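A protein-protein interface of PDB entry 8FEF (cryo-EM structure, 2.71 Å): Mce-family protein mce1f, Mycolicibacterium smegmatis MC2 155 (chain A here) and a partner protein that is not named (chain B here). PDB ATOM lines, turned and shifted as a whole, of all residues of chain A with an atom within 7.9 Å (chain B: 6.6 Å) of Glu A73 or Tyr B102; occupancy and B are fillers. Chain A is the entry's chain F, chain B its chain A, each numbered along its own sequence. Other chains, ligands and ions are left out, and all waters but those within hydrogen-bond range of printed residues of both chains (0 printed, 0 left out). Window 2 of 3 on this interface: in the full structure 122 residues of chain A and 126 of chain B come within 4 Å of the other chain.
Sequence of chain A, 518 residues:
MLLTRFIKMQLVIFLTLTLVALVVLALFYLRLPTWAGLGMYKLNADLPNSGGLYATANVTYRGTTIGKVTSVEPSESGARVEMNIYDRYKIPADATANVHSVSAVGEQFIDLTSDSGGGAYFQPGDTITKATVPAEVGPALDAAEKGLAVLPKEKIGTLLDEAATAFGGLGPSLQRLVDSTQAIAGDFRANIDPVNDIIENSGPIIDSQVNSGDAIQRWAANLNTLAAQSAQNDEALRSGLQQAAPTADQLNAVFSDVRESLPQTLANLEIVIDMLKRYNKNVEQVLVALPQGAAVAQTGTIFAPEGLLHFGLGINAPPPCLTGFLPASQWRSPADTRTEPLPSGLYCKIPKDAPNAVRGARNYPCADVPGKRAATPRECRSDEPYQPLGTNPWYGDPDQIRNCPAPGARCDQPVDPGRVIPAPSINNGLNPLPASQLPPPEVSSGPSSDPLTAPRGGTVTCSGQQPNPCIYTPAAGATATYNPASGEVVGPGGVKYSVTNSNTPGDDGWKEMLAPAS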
ATOM      1  N   ALA A  45       0.439  -0.498  25.234  1.00  0.00           N
ATOM      2  CA  ALA A  45      -0.850  -1.165  25.344  1.00  0.00           C
ATOM      3  C   ALA A  45      -1.319  -1.567  23.954  1.00  0.00           C
ATOM      4  O   ALA A  45      -1.085  -0.846  22.981  1.00  0.00           O
ATOM      5  CB  ALA A  45      -1.893  -0.269  26.020  1.00  0.00           C
ATOM      6  N   LEU A  47      -4.739  -2.629  21.785  1.00  0.00           N
ATOM      7  CA  LEU A  47      -6.184  -2.514  21.815  1.00  0.00           C
ATOM      8  C   LEU A  47      -6.797  -3.197  20.599  1.00  0.00           C
ATOM      9  O   LEU A  47      -6.190  -3.213  19.524  1.00  0.00           O
ATOM     10  CB  LEU A  47      -6.615  -1.042  21.835  1.00  0.00           C
ATOM     11  CG  LEU A  47      -5.866  -0.061  22.737  1.00  0.00           C
ATOM     12  CD1 LEU A  47      -6.327   1.350  22.442  1.00  0.00           C
ATOM     13  CD2 LEU A  47      -6.075  -0.389  24.200  1.00  0.00           C
ATOM     14  N   SER A  50      -8.987   1.522  18.430  1.00  0.00           N
ATOM     15  CA  SER A  50      -8.508   2.724  19.106  1.00  0.00           C
ATOM     16  C   SER A  50      -9.553   3.282  20.062  1.00  0.00           C
ATOM     17  O   SER A  50      -9.222   3.719  21.170  1.00  0.00           O
ATOM     18  CB  SER A  50      -8.118   3.783  18.083  1.00  0.00           C
ATOM     19  OG  SER A  50      -7.612   4.942  18.717  1.00  0.00           O
ATOM     20  N   LEU A  53      -8.996   7.156  20.671  1.00  0.00           N
ATOM     21  CA  LEU A  53      -7.857   7.657  21.426  1.00  0.00           C
ATOM     22  C   LEU A  53      -6.856   8.326  20.493  1.00  0.00           C
ATOM     23  O   LEU A  53      -6.642   7.884  19.363  1.00  0.00           O
ATOM     24  CB  LEU A  53      -7.189   6.515  22.191  1.00  0.00           C
ATOM     25  CG  LEU A  53      -6.211   6.896  23.302  1.00  0.00           C
ATOM     26  CD1 LEU A  53      -6.916   7.705  24.371  1.00  0.00           C
ATOM     27  CD2 LEU A  53      -5.579   5.659  23.904  1.00  0.00           C
ATOM     28  N   ALA A  55      -3.012  10.926  20.372  1.00  0.00           N
ATOM     29  CA  ALA A  55      -1.825  11.365  21.089  1.00  0.00           C
ATOM     30  C   ALA A  55      -2.142  12.615  21.901  1.00  0.00           C
ATOM     31  O   ALA A  55      -3.035  13.392  21.555  1.00  0.00           O
ATOM     32  CB  ALA A  55      -0.679  11.641  20.119  1.00  0.00           C
ATOM     33  N   VAL A  69      -0.767  10.133  26.842  1.00  0.00           N
ATOM     34  CA  VAL A  69      -0.555   9.245  25.705  1.00  0.00           C
ATOM     35  C   VAL A  69       0.451   9.883  24.760  1.00  0.00           C
ATOM     36  O   VAL A  69       0.282  11.032  24.336  1.00  0.00           O
ATOM     37  CB  VAL A  69      -1.881   8.953  24.987  1.00  0.00           C
ATOM     38  CG1 VAL A  69      -1.651   8.046  23.797  1.00  0.00           C
ATOM     39  CG2 VAL A  69      -2.872   8.331  25.940  1.00  0.00           C
ATOM     40  N   THR A  70       1.502   9.139  24.427  1.00  0.00           N
ATOM     41  CA  THR A  70       2.547   9.648  23.548  1.00  0.00           C
ATOM     42  C   THR A  70       2.229   9.410  22.078  1.00  0.00           C
ATOM     43  O   THR A  70       2.393  10.317  21.254  1.00  0.00           O
ATOM     44  CB  THR A  70       3.893   9.011  23.915  1.00  0.00           C
ATOM     45  OG1 THR A  70       4.352   9.551  25.159  1.00  0.00           O
ATOM     46  CG2 THR A  70       4.935   9.273  22.842  1.00  0.00           C
ATOM     47  N   SER A  71       1.756   8.215  21.731  1.00  0.00           N
ATOM     48  CA  SER A  71       1.473   7.902  20.338  1.00  0.00           C
ATOM     49  C   SER A  71       0.416   6.813  20.252  1.00  0.00           C
ATOM     50  O   SER A  71       0.353   5.920  21.099  1.00  0.00           O
ATOM     51  CB  SER A  71       2.734   7.456  19.590  1.00  0.00           C
ATOM     52  OG  SER A  71       3.189   6.202  20.063  1.00  0.00           O
ATOM     53  N   VAL A  72      -0.418   6.902  19.218  1.00  0.00           N
ATOM     54  CA  VAL A  72      -1.386   5.867  18.874  1.00  0.00           C
ATOM     55  C   VAL A  72      -1.187   5.521  17.406  1.00  0.00           C
ATOM     56  O   VAL A  72      -1.229   6.409  16.548  1.00  0.00           O
ATOM     57  CB  VAL A  72      -2.836   6.319  19.133  1.00  0.00           C
ATOM     58  CG1 VAL A  72      -3.805   5.208  18.780  1.00  0.00           C
ATOM     59  CG2 VAL A  72      -3.018   6.739  20.582  1.00  0.00           C
ATOM     60  N   GLU A  73      -0.974   4.242  17.119  1.00  0.00           N
ATOM     61  CA  GLU A  73      -0.673   3.792  15.769  1.00  0.00           C
ATOM     62  C   GLU A  73      -1.523   2.577  15.433  1.00  0.00           C
ATOM     63  O   GLU A  73      -1.966   1.866  16.338  1.00  0.00           O
ATOM     64  CB  GLU A  73       0.820   3.440  15.649  1.00  0.00           C
ATOM     65  CG  GLU A  73       1.510   3.967  14.402  1.00  0.00           C
ATOM     66  CD  GLU A  73       1.485   5.481  14.318  1.00  0.00           C
ATOM     67  OE1 GLU A  73       1.585   6.140  15.374  1.00  0.00           O
ATOM     68  OE2 GLU A  73       1.361   6.014  13.196  1.00  0.00           O
ATOM     69  N   PRO A  74      -1.796   2.326  14.156  1.00  0.00           N
ATOM     70  CA  PRO A  74      -2.502   1.098  13.786  1.00  0.00           C
ATOM     71  C   PRO A  74      -1.571  -0.105  13.759  1.00  0.00           C
ATOM     72  O   PRO A  74      -0.357   0.010  13.585  1.00  0.00           O
ATOM     73  CB  PRO A  74      -3.038   1.402  12.385  1.00  0.00           C
ATOM     74  CG  PRO A  74      -2.080   2.366  11.840  1.00  0.00           C
ATOM     75  CD  PRO A  74      -1.594   3.204  12.991  1.00  0.00           C
ATOM     76  N   SER A  75      -2.175  -1.277  13.935  1.00  0.00           N
ATOM     77  CA  SER A  75      -1.463  -2.541  13.868  1.00  0.00           C
ATOM     78  C   SER A  75      -2.360  -3.557  13.176  1.00  0.00           C
ATOM     79  O   SER A  75      -3.493  -3.256  12.791  1.00  0.00           O
ATOM     80  CB  SER A  75      -1.041  -3.020  15.262  1.00  0.00           C
ATOM     81  OG  SER A  75      -2.164  -3.200  16.104  1.00  0.00           O
ATOM     82  N   GLU A  76      -1.843  -4.774  13.009  1.00  0.00           N
ATOM     83  CA  GLU A  76      -2.633  -5.824  12.378  1.00  0.00           C
ATOM     84  C   GLU A  76      -3.715  -6.353  13.310  1.00  0.00           C
ATOM     85  O   GLU A  76      -4.781  -6.772  12.844  1.00  0.00           O
ATOM     86  CB  GLU A  76      -1.725  -6.963  11.901  1.00  0.00           C
ATOM     87  CG  GLU A  76      -1.001  -7.739  13.001  1.00  0.00           C
ATOM     88  CD  GLU A  76       0.174  -6.982  13.594  1.00  0.00           C
ATOM     89  OE1 GLU A  76       0.599  -5.972  12.995  1.00  0.00           O
ATOM     90  OE2 GLU A  76       0.671  -7.398  14.662  1.00  0.00           O
ATOM     91  N   GLY A  78      -5.120  -4.512  15.819  1.00  0.00           N
ATOM     92  CA  GLY A  78      -5.812  -3.415  16.465  1.00  0.00           C
ATOM     93  C   GLY A  78      -5.026  -2.122  16.451  1.00  0.00           C
ATOM     94  O   GLY A  78      -4.647  -1.630  15.385  1.00  0.00           O
ATOM     95  N   ALA A  79      -4.779  -1.558  17.630  1.00  0.00           N
ATOM     96  CA  ALA A  79      -4.019  -0.328  17.768  1.00  0.00           C
ATOM     97  C   ALA A  79      -2.948  -0.499  18.837  1.00  0.00           C
ATOM     98  O   ALA A  79      -3.141  -1.205  19.830  1.00  0.00           O
ATOM     99  CB  ALA A  79      -4.925   0.855  18.119  1.00  0.00           C
ATOM    100  N   ARG A  80      -1.818   0.162  18.618  1.00  0.00           N
ATOM    101  CA  ARG A  80      -0.693   0.173  19.542  1.00  0.00           C
ATOM    102  C   ARG A  80      -0.610   1.558  20.167  1.00  0.00           C
ATOM    103  O   ARG A  80      -0.523   2.561  19.450  1.00  0.00           O
ATOM    104  CB  ARG A  80       0.606  -0.167  18.811  1.00  0.00           C
ATOM    105  CG  ARG A  80       1.856  -0.133  19.669  1.00  0.00           C
ATOM    106  CD  ARG A  80       1.944  -1.359  20.554  1.00  0.00           C
ATOM    107  NE  ARG A  80       3.279  -1.541  21.109  1.00  0.00           N
ATOM    108  CZ  ARG A  80       3.657  -2.604  21.804  1.00  0.00           C
ATOM    109  NH1 ARG A  80       2.824  -3.600  22.054  1.00  0.00           N
ATOM    110  NH2 ARG A  80       4.905  -2.673  22.258  1.00  0.00           N
ATOM    111  N   VAL A  81      -0.635   1.615  21.495  1.00  0.00           N
ATOM    112  CA  VAL A  81      -0.611   2.871  22.231  1.00  0.00           C
ATOM    113  C   VAL A  81       0.653   2.903  23.076  1.00  0.00           C
ATOM    114  O   VAL A  81       0.916   1.970  23.840  1.00  0.00           O
ATOM    115  CB  VAL A  81      -1.863   3.036  23.110  1.00  0.00           C
ATOM    116  CG1 VAL A  81      -1.770   4.302  23.938  1.00  0.00           C
ATOM    117  CG2 VAL A  81      -3.106   3.059  22.248  1.00  0.00           C
ATOM    118  N   GLU A  82       1.434   3.967  22.930  1.00  0.00           N
ATOM    119  CA  GLU A  82       2.595   4.219  23.770  1.00  0.00           C
ATOM    120  C   GLU A  82       2.330   5.459  24.606  1.00  0.00           C
ATOM    121  O   GLU A  82       1.854   6.472  24.082  1.00  0.00           O
ATOM    122  CB  GLU A  82       3.856   4.406  22.927  1.00  0.00           C
ATOM    123  CG  GLU A  82       4.243   3.184  22.120  1.00  0.00           C
ATOM    124  CD  GLU A  82       5.516   3.395  21.329  1.00  0.00           C
ATOM    125  OE1 GLU A  82       6.033   4.531  21.326  1.00  0.00           O
ATOM    126  OE2 GLU A  82       6.001   2.425  20.709  1.00  0.00           O
ATOM    127  N   PHE B  70      -8.447   3.480  10.219  1.00  0.00           N
ATOM    128  CA  PHE B  70      -8.243   2.039  10.239  1.00  0.00           C
ATOM    129  C   PHE B  70      -8.089   1.615  11.691  1.00  0.00           C
ATOM    130  O   PHE B  70      -7.296   2.210  12.428  1.00  0.00           O
ATOM    131  CB  PHE B  70      -7.016   1.629   9.422  1.00  0.00           C
ATOM    132  CG  PHE B  70      -6.860   0.143   9.269  1.00  0.00           C
ATOM    133  CD1 PHE B  70      -7.624  -0.555   8.351  1.00  0.00           C
ATOM    134  CD2 PHE B  70      -5.949  -0.555  10.043  1.00  0.00           C
ATOM    135  CE1 PHE B  70      -7.486  -1.920   8.209  1.00  0.00           C
ATOM    136  CE2 PHE B  70      -5.807  -1.920   9.904  1.00  0.00           C
ATOM    137  CZ  PHE B  70      -6.577  -2.602   8.986  1.00  0.00           C
ATOM    138  N   VAL B  73      -7.915   4.446  14.221  1.00  0.00           N
ATOM    139  CA  VAL B  73      -6.912   5.508  14.192  1.00  0.00           C
ATOM    140  C   VAL B  73      -6.973   6.200  12.834  1.00  0.00           C
ATOM    141  O   VAL B  73      -7.196   5.537  11.810  1.00  0.00           O
ATOM    142  CB  VAL B  73      -5.501   4.975  14.496  1.00  0.00           C
ATOM    143  CG1 VAL B  73      -5.518   4.067  15.703  1.00  0.00           C
ATOM    144  CG2 VAL B  73      -4.931   4.248  13.318  1.00  0.00           C
ATOM    145  N   PRO B  74      -6.863   7.526  12.781  1.00  0.00           N
ATOM    146  CA  PRO B  74      -6.869   8.206  11.482  1.00  0.00           C
ATOM    147  C   PRO B  74      -5.666   7.805  10.641  1.00  0.00           C
ATOM    148  O   PRO B  74      -4.546   7.682  11.140  1.00  0.00           O
ATOM    149  CB  PRO B  74      -6.826   9.690  11.862  1.00  0.00           C
ATOM    150  CG  PRO B  74      -7.373   9.738  13.247  1.00  0.00           C
ATOM    151  CD  PRO B  74      -6.908   8.477  13.901  1.00  0.00           C
ATOM    152  N   ILE B  75      -5.913   7.606   9.349  1.00  0.00           N
ATOM    153  CA  ILE B  75      -4.883   7.223   8.393  1.00  0.00           C
ATOM    154  C   ILE B  75      -4.960   8.154   7.193  1.00  0.00           C
ATOM    155  O   ILE B  75      -4.093   8.128   6.313  1.00  0.00           O
ATOM    156  CB  ILE B  75      -5.042   5.758   7.951  1.00  0.00           C
ATOM    157  CG1 ILE B  75      -6.376   5.569   7.231  1.00  0.00           C
ATOM    158  CG2 ILE B  75      -4.923   4.814   9.137  1.00  0.00           C
ATOM    159  CD1 ILE B  75      -6.620   4.166   6.768  1.00  0.00           C
ATOM    160  N   GLY B  76      -6.000   8.974   7.146  1.00  0.00           N
ATOM    161  CA  GLY B  76      -6.179   9.867   6.022  1.00  0.00           C
ATOM    162  C   GLY B  76      -7.365  10.774   6.237  1.00  0.00           C
ATOM    163  O   GLY B  76      -7.832  10.953   7.362  1.00  0.00           O
ATOM    164  N   VAL B  98      -5.058   8.814   1.521  1.00  0.00           N
ATOM    165  CA  VAL B  98      -4.538   7.979   2.595  1.00  0.00           C
ATOM    166  C   VAL B  98      -3.017   7.992   2.547  1.00  0.00           C
ATOM    167  O   VAL B  98      -2.420   7.911   1.467  1.00  0.00           O
ATOM    168  CB  VAL B  98      -5.078   6.535   2.496  1.00  0.00           C
ATOM    169  CG1 VAL B  98      -4.547   5.678   3.633  1.00  0.00           C
ATOM    170  CG2 VAL B  98      -6.597   6.534   2.501  1.00  0.00           C
ATOM    171  N   ASP B  99      -2.399   8.107   3.716  1.00  0.00           N
ATOM    172  CA  ASP B  99      -0.949   8.004   3.840  1.00  0.00           C
ATOM    173  C   ASP B  99      -0.516   6.591   3.466  1.00  0.00           C
ATOM    174  O   ASP B  99      -0.999   5.628   4.075  1.00  0.00           O
ATOM    175  CB  ASP B  99      -0.531   8.340   5.270  1.00  0.00           C
ATOM    176  CG  ASP B  99       0.931   8.735   5.387  1.00  0.00           C
ATOM    177  OD1 ASP B  99       1.768   8.216   4.623  1.00  0.00           O
ATOM    178  OD2 ASP B  99       1.244   9.573   6.260  1.00  0.00           O
ATOM    179  N   PRO B 100       0.378   6.414   2.487  1.00  0.00           N
ATOM    180  CA  PRO B 100       0.725   5.059   2.029  1.00  0.00           C
ATOM    181  C   PRO B 100       1.489   4.218   3.040  1.00  0.00           C
ATOM    182  O   PRO B 100       1.798   3.061   2.735  1.00  0.00           O
ATOM    183  CB  PRO B 100       1.578   5.324   0.780  1.00  0.00           C
ATOM    184  CG  PRO B 100       2.100   6.703   0.961  1.00  0.00           C
ATOM    185  CD  PRO B 100       1.014   7.453   1.660  1.00  0.00           C
ATOM    186  N   LYS B 101       1.817   4.749   4.220  1.00  0.00           N
ATOM    187  CA  LYS B 101       2.447   3.926   5.248  1.00  0.00           C
ATOM    188  C   LYS B 101       1.519   2.806   5.695  1.00  0.00           C
ATOM    189  O   LYS B 101       1.965   1.681   5.952  1.00  0.00           O
ATOM    190  CB  LYS B 101       2.844   4.782   6.449  1.00  0.00           C
ATOM    191  CG  LYS B 101       3.663   6.010   6.119  1.00  0.00           C
ATOM    192  CD  LYS B 101       4.057   6.744   7.390  1.00  0.00           C
ATOM    193  CE  LYS B 101       2.845   7.020   8.266  1.00  0.00           C
ATOM    194  NZ  LYS B 101       3.223   7.647   9.561  1.00  0.00           N
ATOM    195  N   TYR B 102       0.224   3.096   5.798  1.00  0.00           N
ATOM    196  CA  TYR B 102      -0.753   2.150   6.309  1.00  0.00           C
ATOM    197  C   TYR B 102      -1.375   1.278   5.228  1.00  0.00           C
ATOM    198  O   TYR B 102      -2.116   0.349   5.561  1.00  0.00           O
ATOM    199  CB  TYR B 102      -1.862   2.900   7.049  1.00  0.00           C
ATOM    200  CG  TYR B 102      -1.366   4.055   7.885  1.00  0.00           C
ATOM    201  CD1 TYR B 102      -0.690   3.833   9.073  1.00  0.00           C
ATOM    202  CD2 TYR B 102      -1.580   5.365   7.488  1.00  0.00           C
ATOM    203  CE1 TYR B 102      -0.241   4.882   9.846  1.00  0.00           C
ATOM    204  CE2 TYR B 102      -1.136   6.422   8.255  1.00  0.00           C
ATOM    205  CZ  TYR B 102      -0.466   6.175   9.432  1.00  0.00           C
ATOM    206  OH  TYR B 102      -0.019   7.225  10.198  1.00  0.00           O
ATOM    207  N   LEU B 103      -1.098   1.556   3.950  1.00  0.00           N
ATOM    208  CA  LEU B 103      -1.711   0.789   2.870  1.00  0.00           C
ATOM    209  C   LEU B 103      -1.301  -0.677   2.923  1.00  0.00           C
ATOM    210  O   LEU B 103      -2.126  -1.568   2.691  1.00  0.00           O
ATOM    211  CB  LEU B 103      -1.345   1.398   1.517  1.00  0.00           C
ATOM    212  CG  LEU B 103      -2.518   1.952   0.709  1.00  0.00           C
ATOM    213  CD1 LEU B 103      -3.327   2.914   1.550  1.00  0.00           C
ATOM    214  CD2 LEU B 103      -2.022   2.631  -0.555  1.00  0.00           C
ATOM    215  N   ASP B 104      -0.030  -0.948   3.225  1.00  0.00           N
ATOM    216  CA  ASP B 104       0.426  -2.323   3.376  1.00  0.00           C
ATOM    217  C   ASP B 104      -0.174  -3.010   4.596  1.00  0.00           C
ATOM    218  O   ASP B 104      -0.086  -4.239   4.703  1.00  0.00           O
ATOM    219  CB  ASP B 104       1.954  -2.360   3.455  1.00  0.00           C
ATOM    220  CG  ASP B 104       2.519  -3.751   3.226  1.00  0.00           C
ATOM    221  OD1 ASP B 104       2.591  -4.179   2.055  1.00  0.00           O
ATOM    222  OD2 ASP B 104       2.887  -4.416   4.217  1.00  0.00           O
ATOM    223  N   LEU B 105      -0.784  -2.256   5.510  1.00  0.00           N
ATOM    224  CA  LEU B 105      -1.402  -2.822   6.700  1.00  0.00           C
ATOM    225  C   LEU B 105      -2.889  -3.105   6.525  1.00  0.00           C
ATOM    226  O   LEU B 105      -3.451  -3.893   7.294  1.00  0.00           O
ATOM    227  CB  LEU B 105      -1.194  -1.873   7.886  1.00  0.00           C
ATOM    228  CG  LEU B 105      -1.444  -2.384   9.304  1.00  0.00           C
ATOM    229  CD1 LEU B 105      -0.489  -3.514   9.640  1.00  0.00           C
ATOM    230  CD2 LEU B 105      -1.305  -1.250  10.303  1.00  0.00           C
ATOM    231  N   ILE B 106      -3.531  -2.503   5.529  1.00  0.00           N
ATOM    232  CA  ILE B 106      -4.970  -2.638   5.325  1.00  0.00           C
ATOM    233  C   ILE B 106      -5.213  -3.832   4.407  1.00  0.00           C
ATOM    234  O   ILE B 106      -4.704  -3.836   3.275  1.00  0.00           O
ATOM    235  CB  ILE B 106      -5.577  -1.365   4.728  1.00  0.00           C
ATOM    236  CG1 ILE B 106      -5.292  -0.161   5.623  1.00  0.00           C
ATOM    237  CG2 ILE B 106      -7.074  -1.532   4.542  1.00  0.00           C
ATOM    238  CD1 ILE B 106      -5.703   1.146   5.001  1.00  0.00           C
ATOM    239  N   PRO B 107      -5.970  -4.838   4.836  1.00  0.00           N
ATOM    240  CA  PRO B 107      -6.277  -5.965   3.952  1.00  0.00           C
ATOM    241  C   PRO B 107      -7.185  -5.551   2.805  1.00  0.00           C
ATOM    242  O   PRO B 107      -7.898  -4.548   2.864  1.00  0.00           O
ATOM    243  CB  PRO B 107      -6.975  -6.964   4.877  1.00  0.00           C
ATOM    244  CG  PRO B 107      -7.530  -6.130   5.978  1.00  0.00           C
ATOM    245  CD  PRO B 107      -6.556  -5.008   6.176  1.00  0.00           C
ATOM    246  N   ARG B 137      -3.298  -6.414  -0.833  1.00  0.00           N
ATOM    247  CA  ARG B 137      -3.368  -5.205  -0.031  1.00  0.00           C
ATOM    248  C   ARG B 137      -4.161  -4.122  -0.752  1.00  0.00           C
ATOM    249  O   ARG B 137      -4.232  -4.093  -1.985  1.00  0.00           O
ATOM    250  CB  ARG B 137      -1.965  -4.696   0.310  1.00  0.00           C
ATOM    251  CG  ARG B 137      -1.596  -4.874   1.772  1.00  0.00           C
ATOM    252  CD  ARG B 137      -2.069  -6.212   2.310  1.00  0.00           C
ATOM    253  NE  ARG B 137      -2.055  -6.248   3.767  1.00  0.00           N
ATOM    254  CZ  ARG B 137      -2.643  -7.185   4.497  1.00  0.00           C
ATOM    255  NH1 ARG B 137      -3.308  -8.181   3.937  1.00  0.00           N
ATOM    256  NH2 ARG B 137      -2.567  -7.116   5.823  1.00  0.00           N
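Ser A50 touches Val B73. CG1 of Val B73 touches CG1 of Val A72, at 3.7 Å. OH of Tyr B102 touches OE2 of Glu A73, at 3.5 Å. CD of Pro A74 touches CG2 of Val B73 (3.5 Å). Pro A74 touches Tyr B102 (CG to CD1, 3.4 Å). CD2 of Leu B105 touches O of Pro A74, at 3.6 Å. Ser A75 touches Phe B70 (O to CE2, 3.9 Å). Leu B105 touches Ser A75. Leu B105 touches Glu A76.
Glu A73 touches just one residue of chain B: Tyr B102. Tyr B102 touches just these residues of chain A: Glu A73 and Pro A74. Of the printed residues of chain A, Leu B105 touches Pro A74 (3.6 Å), Ser A75 (3.7 Å) and Glu A76 (3.8 Å). Printed residues of chain A within 4 Å of Val B73: Ser A50 (3.5 Å), Val A72 (3.7 Å) and Pro A74 (3.5 Å). The nearest residue of chain A that does not touch Tyr B102 is Val A72 (6.5 Å).
Hydrophobic or aromatic side chains of chain A that line the printed part of chain B: Val A72 and Pro A74. Hydrophobic or aromatic side chains of chain B within 4 Å of the printed part of chain A: Phe B70, Val B73, Tyr B102 and Leu B105.
The side-chain hydroxyl of Tyr B102 lies within hydrogen-bond range of the side-chain amino group of Lys B101, 3.3 Å away. O of Leu A53 lies within hydrogen-bond range of OG of Ser A50 (3.2 Å). The backbone NH (N) of Arg A80 sits at hydrogen-bond distance from the backbone carbonyl oxygen (O) of Glu A73, 2.9 Å away. The side-chain hydroxyl of Ser A75 is in hydrogen-bond range of the backbone carbonyl oxygen of Gly A78. N of Ala A79 sits at hydrogen-bond distance from OG of Ser A75 (3.4 Å).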
